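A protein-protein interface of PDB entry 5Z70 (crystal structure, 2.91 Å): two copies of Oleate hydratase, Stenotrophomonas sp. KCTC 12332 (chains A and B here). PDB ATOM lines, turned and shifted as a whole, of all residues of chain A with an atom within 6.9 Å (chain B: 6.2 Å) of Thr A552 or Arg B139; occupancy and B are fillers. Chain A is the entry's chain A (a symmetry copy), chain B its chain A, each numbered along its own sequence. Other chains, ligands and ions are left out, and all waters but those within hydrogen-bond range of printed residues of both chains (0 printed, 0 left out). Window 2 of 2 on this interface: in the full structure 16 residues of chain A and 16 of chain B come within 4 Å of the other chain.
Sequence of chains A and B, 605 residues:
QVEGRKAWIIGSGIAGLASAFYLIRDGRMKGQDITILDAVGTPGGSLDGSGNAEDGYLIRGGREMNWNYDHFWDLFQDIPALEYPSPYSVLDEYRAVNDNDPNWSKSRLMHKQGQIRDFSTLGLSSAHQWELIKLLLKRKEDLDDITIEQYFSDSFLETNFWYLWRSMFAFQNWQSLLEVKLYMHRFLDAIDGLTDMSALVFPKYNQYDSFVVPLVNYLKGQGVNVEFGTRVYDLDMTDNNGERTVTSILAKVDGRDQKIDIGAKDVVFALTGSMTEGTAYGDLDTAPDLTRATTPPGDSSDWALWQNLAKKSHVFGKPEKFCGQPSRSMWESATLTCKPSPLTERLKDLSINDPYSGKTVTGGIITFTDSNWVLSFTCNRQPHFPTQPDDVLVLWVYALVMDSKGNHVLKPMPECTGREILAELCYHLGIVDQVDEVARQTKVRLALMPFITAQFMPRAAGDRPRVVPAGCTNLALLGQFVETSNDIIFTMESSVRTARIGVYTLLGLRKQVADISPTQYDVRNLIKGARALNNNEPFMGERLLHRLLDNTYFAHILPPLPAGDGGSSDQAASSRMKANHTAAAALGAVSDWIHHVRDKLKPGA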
ATOM      1  N   ARG A 547      11.711  33.064  10.835  1.00  0.00           N
ATOM      2  CA  ARG A 547      11.213  32.926   9.468  1.00  0.00           C
ATOM      3  C   ARG A 547      11.810  31.715   8.754  1.00  0.00           C
ATOM      4  O   ARG A 547      11.142  31.106   7.912  1.00  0.00           O
ATOM      5  CB  ARG A 547      11.469  34.211   8.680  1.00  0.00           C
ATOM      6  CG  ARG A 547      10.884  34.183   7.275  1.00  0.00           C
ATOM      7  CD  ARG A 547      10.650  35.576   6.716  1.00  0.00           C
ATOM      8  NE  ARG A 547       9.624  36.286   7.475  1.00  0.00           N
ATOM      9  CZ  ARG A 547       9.103  37.457   7.122  1.00  0.00           C
ATOM     10  NH1 ARG A 547       9.503  38.057   6.010  1.00  0.00           N
ATOM     11  NH2 ARG A 547       8.173  38.024   7.880  1.00  0.00           N
ATOM     12  N   LEU A 548      13.050  31.339   9.075  1.00  0.00           N
ATOM     13  CA  LEU A 548      13.640  30.174   8.420  1.00  0.00           C
ATOM     14  C   LEU A 548      13.237  28.867   9.090  1.00  0.00           C
ATOM     15  O   LEU A 548      13.257  27.816   8.435  1.00  0.00           O
ATOM     16  CB  LEU A 548      15.166  30.267   8.372  1.00  0.00           C
ATOM     17  CG  LEU A 548      15.808  31.196   7.338  1.00  0.00           C
ATOM     18  CD1 LEU A 548      15.863  32.619   7.831  1.00  0.00           C
ATOM     19  CD2 LEU A 548      17.196  30.700   6.961  1.00  0.00           C
ATOM     20  N   LEU A 549      12.884  28.895  10.380  1.00  0.00           N
ATOM     21  CA  LEU A 549      12.727  27.661  11.139  1.00  0.00           C
ATOM     22  C   LEU A 549      11.315  27.374  11.643  1.00  0.00           C
ATOM     23  O   LEU A 549      11.077  26.269  12.138  1.00  0.00           O
ATOM     24  CB  LEU A 549      13.695  27.649  12.334  1.00  0.00           C
ATOM     25  CG  LEU A 549      15.201  27.663  11.996  1.00  0.00           C
ATOM     26  CD1 LEU A 549      16.034  27.372  13.231  1.00  0.00           C
ATOM     27  CD2 LEU A 549      15.529  26.680  10.881  1.00  0.00           C
ATOM     28  N   ASP A 550      10.370  28.310  11.530  1.00  0.00           N
ATOM     29  CA  ASP A 550       9.060  28.101  12.152  1.00  0.00           C
ATOM     30  C   ASP A 550       8.298  26.932  11.536  1.00  0.00           C
ATOM     31  O   ASP A 550       7.443  26.336  12.200  1.00  0.00           O
ATOM     32  CB  ASP A 550       8.218  29.374  12.070  1.00  0.00           C
ATOM     33  CG  ASP A 550       8.633  30.419  13.085  1.00  0.00           C
ATOM     34  OD1 ASP A 550       9.087  30.044  14.188  1.00  0.00           O
ATOM     35  OD2 ASP A 550       8.501  31.618  12.774  1.00  0.00           O
ATOM     36  N   ASN A 551       8.565  26.597  10.277  1.00  0.00           N
ATOM     37  CA  ASN A 551       7.866  25.504   9.612  1.00  0.00           C
ATOM     38  C   ASN A 551       8.797  24.331   9.321  1.00  0.00           C
ATOM     39  O   ASN A 551       8.692  23.671   8.283  1.00  0.00           O
ATOM     40  CB  ASN A 551       7.212  25.989   8.324  1.00  0.00           C
ATOM     41  CG  ASN A 551       5.934  26.759   8.574  1.00  0.00           C
ATOM     42  OD1 ASN A 551       4.975  26.233   9.142  1.00  0.00           O
ATOM     43  ND2 ASN A 551       5.906  28.013   8.137  1.00  0.00           N
ATOM     44  N   THR A 552       9.717  24.058  10.245  1.00  0.00           N
ATOM     45  CA  THR A 552      10.733  23.031  10.083  1.00  0.00           C
ATOM     46  C   THR A 552      10.791  22.158  11.332  1.00  0.00           C
ATOM     47  O   THR A 552      10.076  22.378  12.316  1.00  0.00           O
ATOM     48  CB  THR A 552      12.119  23.641   9.817  1.00  0.00           C
ATOM     49  OG1 THR A 552      12.644  24.182  11.036  1.00  0.00           O
ATOM     50  CG2 THR A 552      12.050  24.734   8.754  1.00  0.00           C
ATOM     51  N   TYR A 553      11.662  21.147  11.266  1.00  0.00           N
ATOM     52  CA  TYR A 553      11.931  20.280  12.409  1.00  0.00           C
ATOM     53  C   TYR A 553      12.431  21.068  13.612  1.00  0.00           C
ATOM     54  O   TYR A 553      12.248  20.636  14.756  1.00  0.00           O
ATOM     55  CB  TYR A 553      12.948  19.211  12.001  1.00  0.00           C
ATOM     56  CG  TYR A 553      13.389  18.257  13.094  1.00  0.00           C
ATOM     57  CD1 TYR A 553      14.474  18.560  13.911  1.00  0.00           C
ATOM     58  CD2 TYR A 553      12.746  17.042  13.289  1.00  0.00           C
ATOM     59  CE1 TYR A 553      14.893  17.691  14.901  1.00  0.00           C
ATOM     60  CE2 TYR A 553      13.158  16.165  14.276  1.00  0.00           C
ATOM     61  CZ  TYR A 553      14.233  16.494  15.079  1.00  0.00           C
ATOM     62  OH  TYR A 553      14.648  15.626  16.064  1.00  0.00           O
ATOM     63  N   PHE A 554      13.063  22.219  13.378  1.00  0.00           N
ATOM     64  CA  PHE A 554      13.767  22.968  14.411  1.00  0.00           C
ATOM     65  C   PHE A 554      12.958  24.144  14.950  1.00  0.00           C
ATOM     66  O   PHE A 554      13.539  25.146  15.376  1.00  0.00           O
ATOM     67  CB  PHE A 554      15.107  23.463  13.868  1.00  0.00           C
ATOM     68  CG  PHE A 554      16.058  22.362  13.508  1.00  0.00           C
ATOM     69  CD1 PHE A 554      16.842  21.763  14.476  1.00  0.00           C
ATOM     70  CD2 PHE A 554      16.155  21.913  12.204  1.00  0.00           C
ATOM     71  CE1 PHE A 554      17.717  20.746  14.146  1.00  0.00           C
ATOM     72  CE2 PHE A 554      17.026  20.894  11.871  1.00  0.00           C
ATOM     73  CZ  PHE A 554      17.807  20.311  12.845  1.00  0.00           C
ATOM     74  N   ALA A 555      11.628  24.061  14.915  1.00  0.00           N
ATOM     75  CA  ALA A 555      10.819  25.139  15.474  1.00  0.00           C
ATOM     76  C   ALA A 555      11.001  25.258  16.985  1.00  0.00           C
ATOM     77  O   ALA A 555      10.930  26.365  17.534  1.00  0.00           O
ATOM     78  CB  ALA A 555       9.345  24.922  15.134  1.00  0.00           C
ATOM     79  N   HIS A 556      11.238  24.136  17.671  1.00  0.00           N
ATOM     80  CA  HIS A 556      11.250  24.135  19.130  1.00  0.00           C
ATOM     81  C   HIS A 556      12.501  24.770  19.723  1.00  0.00           C
ATOM     82  O   HIS A 556      12.481  25.151  20.898  1.00  0.00           O
ATOM     83  CB  HIS A 556      11.122  22.704  19.654  1.00  0.00           C
ATOM     84  CG  HIS A 556      12.148  21.767  19.100  1.00  0.00           C
ATOM     85  ND1 HIS A 556      12.016  21.152  17.874  1.00  0.00           N
ATOM     86  CD2 HIS A 556      13.331  21.344  19.604  1.00  0.00           C
ATOM     87  CE1 HIS A 556      13.070  20.387  17.650  1.00  0.00           C
ATOM     88  NE2 HIS A 556      13.884  20.487  18.685  1.00  0.00           N
ATOM     89  N   LEU B 135      15.971  17.399   3.736  1.00  0.00           N
ATOM     90  CA  LEU B 135      15.368  16.292   4.472  1.00  0.00           C
ATOM     91  C   LEU B 135      15.429  16.537   5.975  1.00  0.00           C
ATOM     92  O   LEU B 135      14.443  16.328   6.690  1.00  0.00           O
ATOM     93  CB  LEU B 135      16.069  14.980   4.105  1.00  0.00           C
ATOM     94  CG  LEU B 135      15.705  13.741   4.924  1.00  0.00           C
ATOM     95  CD1 LEU B 135      14.267  13.332   4.654  1.00  0.00           C
ATOM     96  CD2 LEU B 135      16.658  12.590   4.623  1.00  0.00           C
ATOM     97  N   LEU B 137      15.350  19.236   7.520  1.00  0.00           N
ATOM     98  CA  LEU B 137      14.515  20.355   7.933  1.00  0.00           C
ATOM     99  C   LEU B 137      13.023  20.054   7.876  1.00  0.00           C
ATOM    100  O   LEU B 137      12.234  20.827   8.427  1.00  0.00           O
ATOM    101  CB  LEU B 137      14.804  21.584   7.065  1.00  0.00           C
ATOM    102  CG  LEU B 137      16.221  22.157   7.111  1.00  0.00           C
ATOM    103  CD1 LEU B 137      16.387  23.266   6.079  1.00  0.00           C
ATOM    104  CD2 LEU B 137      16.546  22.663   8.507  1.00  0.00           C
ATOM    105  N   LYS B 138      12.615  18.963   7.236  1.00  0.00           N
ATOM    106  CA  LYS B 138      11.194  18.670   7.130  1.00  0.00           C
ATOM    107  C   LYS B 138      10.630  18.212   8.470  1.00  0.00           C
ATOM    108  O   LYS B 138      11.335  17.645   9.309  1.00  0.00           O
ATOM    109  CB  LYS B 138      10.941  17.604   6.064  1.00  0.00           C
ATOM    110  CG  LYS B 138      11.305  18.049   4.662  1.00  0.00           C
ATOM    111  CD  LYS B 138      10.512  17.288   3.614  1.00  0.00           C
ATOM    112  CE  LYS B 138      10.182  18.181   2.427  1.00  0.00           C
ATOM    113  NZ  LYS B 138       9.357  19.352   2.842  1.00  0.00           N
ATOM    114  N   ARG B 139       9.344  18.477   8.667  1.00  0.00           N
ATOM    115  CA  ARG B 139       8.651  18.014   9.857  1.00  0.00           C
ATOM    116  C   ARG B 139       8.273  16.546   9.706  1.00  0.00           C
ATOM    117  O   ARG B 139       7.973  16.069   8.608  1.00  0.00           O
ATOM    118  CB  ARG B 139       7.397  18.856  10.111  1.00  0.00           C
ATOM    119  CG  ARG B 139       7.664  20.345  10.292  1.00  0.00           C
ATOM    120  CD  ARG B 139       6.417  21.081  10.763  1.00  0.00           C
ATOM    121  NE  ARG B 139       5.415  21.189   9.705  1.00  0.00           N
ATOM    122  CZ  ARG B 139       4.207  20.638   9.757  1.00  0.00           C
ATOM    123  NH1 ARG B 139       3.839  19.938  10.822  1.00  0.00           N
ATOM    124  NH2 ARG B 139       3.363  20.793   8.745  1.00  0.00           N
ATOM    125  N   LYS B 140       8.298  15.824  10.828  1.00  0.00           N
ATOM    126  CA  LYS B 140       7.924  14.415  10.803  1.00  0.00           C
ATOM    127  C   LYS B 140       6.446  14.234  10.478  1.00  0.00           C
ATOM    128  O   LYS B 140       6.050  13.185   9.958  1.00  0.00           O
ATOM    129  CB  LYS B 140       8.264  13.763  12.145  1.00  0.00           C
ATOM    130  CG  LYS B 140       9.753  13.522  12.356  1.00  0.00           C
ATOM    131  CD  LYS B 140      10.111  12.057  12.146  1.00  0.00           C
ATOM    132  CE  LYS B 140      11.605  11.871  11.930  1.00  0.00           C
ATOM    133  NZ  LYS B 140      12.421  12.436  13.040  1.00  0.00           N
ATOM    134  N   GLU B 141       5.621  15.239  10.782  1.00  0.00           N
ATOM    135  CA  GLU B 141       4.200  15.167  10.470  1.00  0.00           C
ATOM    136  C   GLU B 141       3.925  15.234   8.974  1.00  0.00           C
ATOM    137  O   GLU B 141       2.825  14.869   8.546  1.00  0.00           O
ATOM    138  CB  GLU B 141       3.442  16.301  11.167  1.00  0.00           C
ATOM    139  CG  GLU B 141       3.708  16.428  12.659  1.00  0.00           C
ATOM    140  CD  GLU B 141       4.911  17.308  12.956  1.00  0.00           C
ATOM    141  OE1 GLU B 141       4.796  18.542  12.801  1.00  0.00           O
ATOM    142  OE2 GLU B 141       5.976  16.767  13.324  1.00  0.00           O
ATOM    143  N   ASP B 142       4.886  15.692   8.174  1.00  0.00           N
ATOM    144  CA  ASP B 142       4.676  15.910   6.749  1.00  0.00           C
ATOM    145  C   ASP B 142       5.327  14.845   5.873  1.00  0.00           C
ATOM    146  O   ASP B 142       5.453  15.052   4.662  1.00  0.00           O
ATOM    147  CB  ASP B 142       5.207  17.291   6.351  1.00  0.00           C
ATOM    148  CG  ASP B 142       4.529  18.423   7.102  1.00  0.00           C
ATOM    149  OD1 ASP B 142       3.389  18.236   7.578  1.00  0.00           O
ATOM    150  OD2 ASP B 142       5.143  19.504   7.222  1.00  0.00           O
ATOM    151  N   LEU B 143       5.738  13.714   6.442  1.00  0.00           N
ATOM    152  CA  LEU B 143       6.421  12.672   5.682  1.00  0.00           C
ATOM    153  C   LEU B 143       5.735  11.324   5.847  1.00  0.00           C
ATOM    154  O   LEU B 143       6.391  10.287   5.982  1.00  0.00           O
ATOM    155  CB  LEU B 143       7.889  12.576   6.090  1.00  0.00           C
ATOM    156  CG  LEU B 143       8.781  13.780   5.781  1.00  0.00           C
ATOM    157  CD1 LEU B 143      10.194  13.523   6.277  1.00  0.00           C
ATOM    158  CD2 LEU B 143       8.783  14.101   4.294  1.00  0.00           C
ATOM    159  N   LEU B 178      11.369   8.085   6.751  1.00  0.00           N
ATOM    160  CA  LEU B 178      11.548   8.504   8.138  1.00  0.00           C
ATOM    161  C   LEU B 178      12.797   7.904   8.775  1.00  0.00           C
ATOM    162  O   LEU B 178      13.431   8.547   9.619  1.00  0.00           O
ATOM    163  CB  LEU B 178      10.308   8.134   8.952  1.00  0.00           C
ATOM    164  CG  LEU B 178       9.050   8.954   8.664  1.00  0.00           C
ATOM    165  CD1 LEU B 178       7.978   8.656   9.694  1.00  0.00           C
ATOM    166  CD2 LEU B 178       9.366  10.443   8.644  1.00  0.00           C
ATOM    167  N   LYS B 181      15.863   9.836   7.619  1.00  0.00           N
ATOM    168  CA  LYS B 181      15.854  11.110   8.331  1.00  0.00           C
ATOM    169  C   LYS B 181      16.307  10.936   9.776  1.00  0.00           C
ATOM    170  O   LYS B 181      17.176  11.672  10.258  1.00  0.00           O
ATOM    171  CB  LYS B 181      14.458  11.730   8.272  1.00  0.00           C
ATOM    172  CG  LYS B 181      14.327  13.040   9.025  1.00  0.00           C
ATOM    173  CD  LYS B 181      12.894  13.539   9.001  1.00  0.00           C
ATOM    174  CE  LYS B 181      12.776  14.893   9.672  1.00  0.00           C
ATOM    175  NZ  LYS B 181      13.809  15.852   9.183  1.00  0.00           N
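Of the 10 printed residues of chain A, 3 touch a printed residue of chain B.
Printed residues of chain A that touch a printed residue of chain B: Thr A552, Tyr A553 and Phe A554.
Among the printed residues, no Asp or Glu carboxylate lies within 4 Å of a Lys or Arg side-chain nitrogen of the other chain.
The backbone carbonyl oxygen of Leu B137 lies within hydrogen-bond range of the backbone NH of Tyr A553 (2.9 Å).
No position is printed for both chains.
Of the 6 pairs that touch across the chains among the printed residues, none has its exchanged pair printed and touching as well.
Of the printed residues of chain B, Thr A552 touches Leu B137 and Arg B139.
Of the printed residues of chain B, Tyr A553 touches Leu B137 (2.9 Å), Lys B138 (3.5 Å) and Lys B140 (3.997 Å).
His A556 touches none of the printed residues of chain B.
Of the printed residues of chain A, Leu B137 touches Thr A552, Tyr A553 and Phe A554.
Of the printed residues of chain A, Arg B139 touches Thr A552.
Asp B142 touches none of the printed residues of chain A.
The nearest printed residue of chain A that does not touch Arg B139 is Asn A551 (4.02 Å).
The nearest printed residue of chain B that does not touch Tyr A553 is Arg B139 (4.2 Å).
Among the printed residues, pairs that only touch across the chains: Thr A552 with Leu B137 (3.1 Å), Thr A552 with Arg B139 (3.7 Å), Tyr A553 with Lys B138 (3.5 Å), Tyr A553 with Lys B140 (3.997 Å) and Phe A554 with Leu B137 (3.8 Å).
The backbone carbonyl oxygen (O) of Lys B138 is in hydrogen-bond range of the side-chain amino group (NZ) of Lys B181.
The guanidinium group (NH1) of Arg B139 is in salt-bridge range of the side-chain carboxylate (OE1) of Glu B141, 2.6 Å away.
The side-chain carboxylate (OD2) of Asp B142 lies within salt-bridge range of the guanidinium group (NH2) of Arg B139.
The backbone carbonyl oxygen of Leu A549 lies within hydrogen-bond range of the side-chain hydroxyl of Thr A552, 2.8 Å away.
The backbone NH of Phe A554 lies close to the side-chain hydroxyl of Thr A552 (3.1 Å).
A ring nitrogen (ND1) of His A556 lies close to the backbone carbonyl oxygen (O) of Tyr A553 (3.2 Å).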
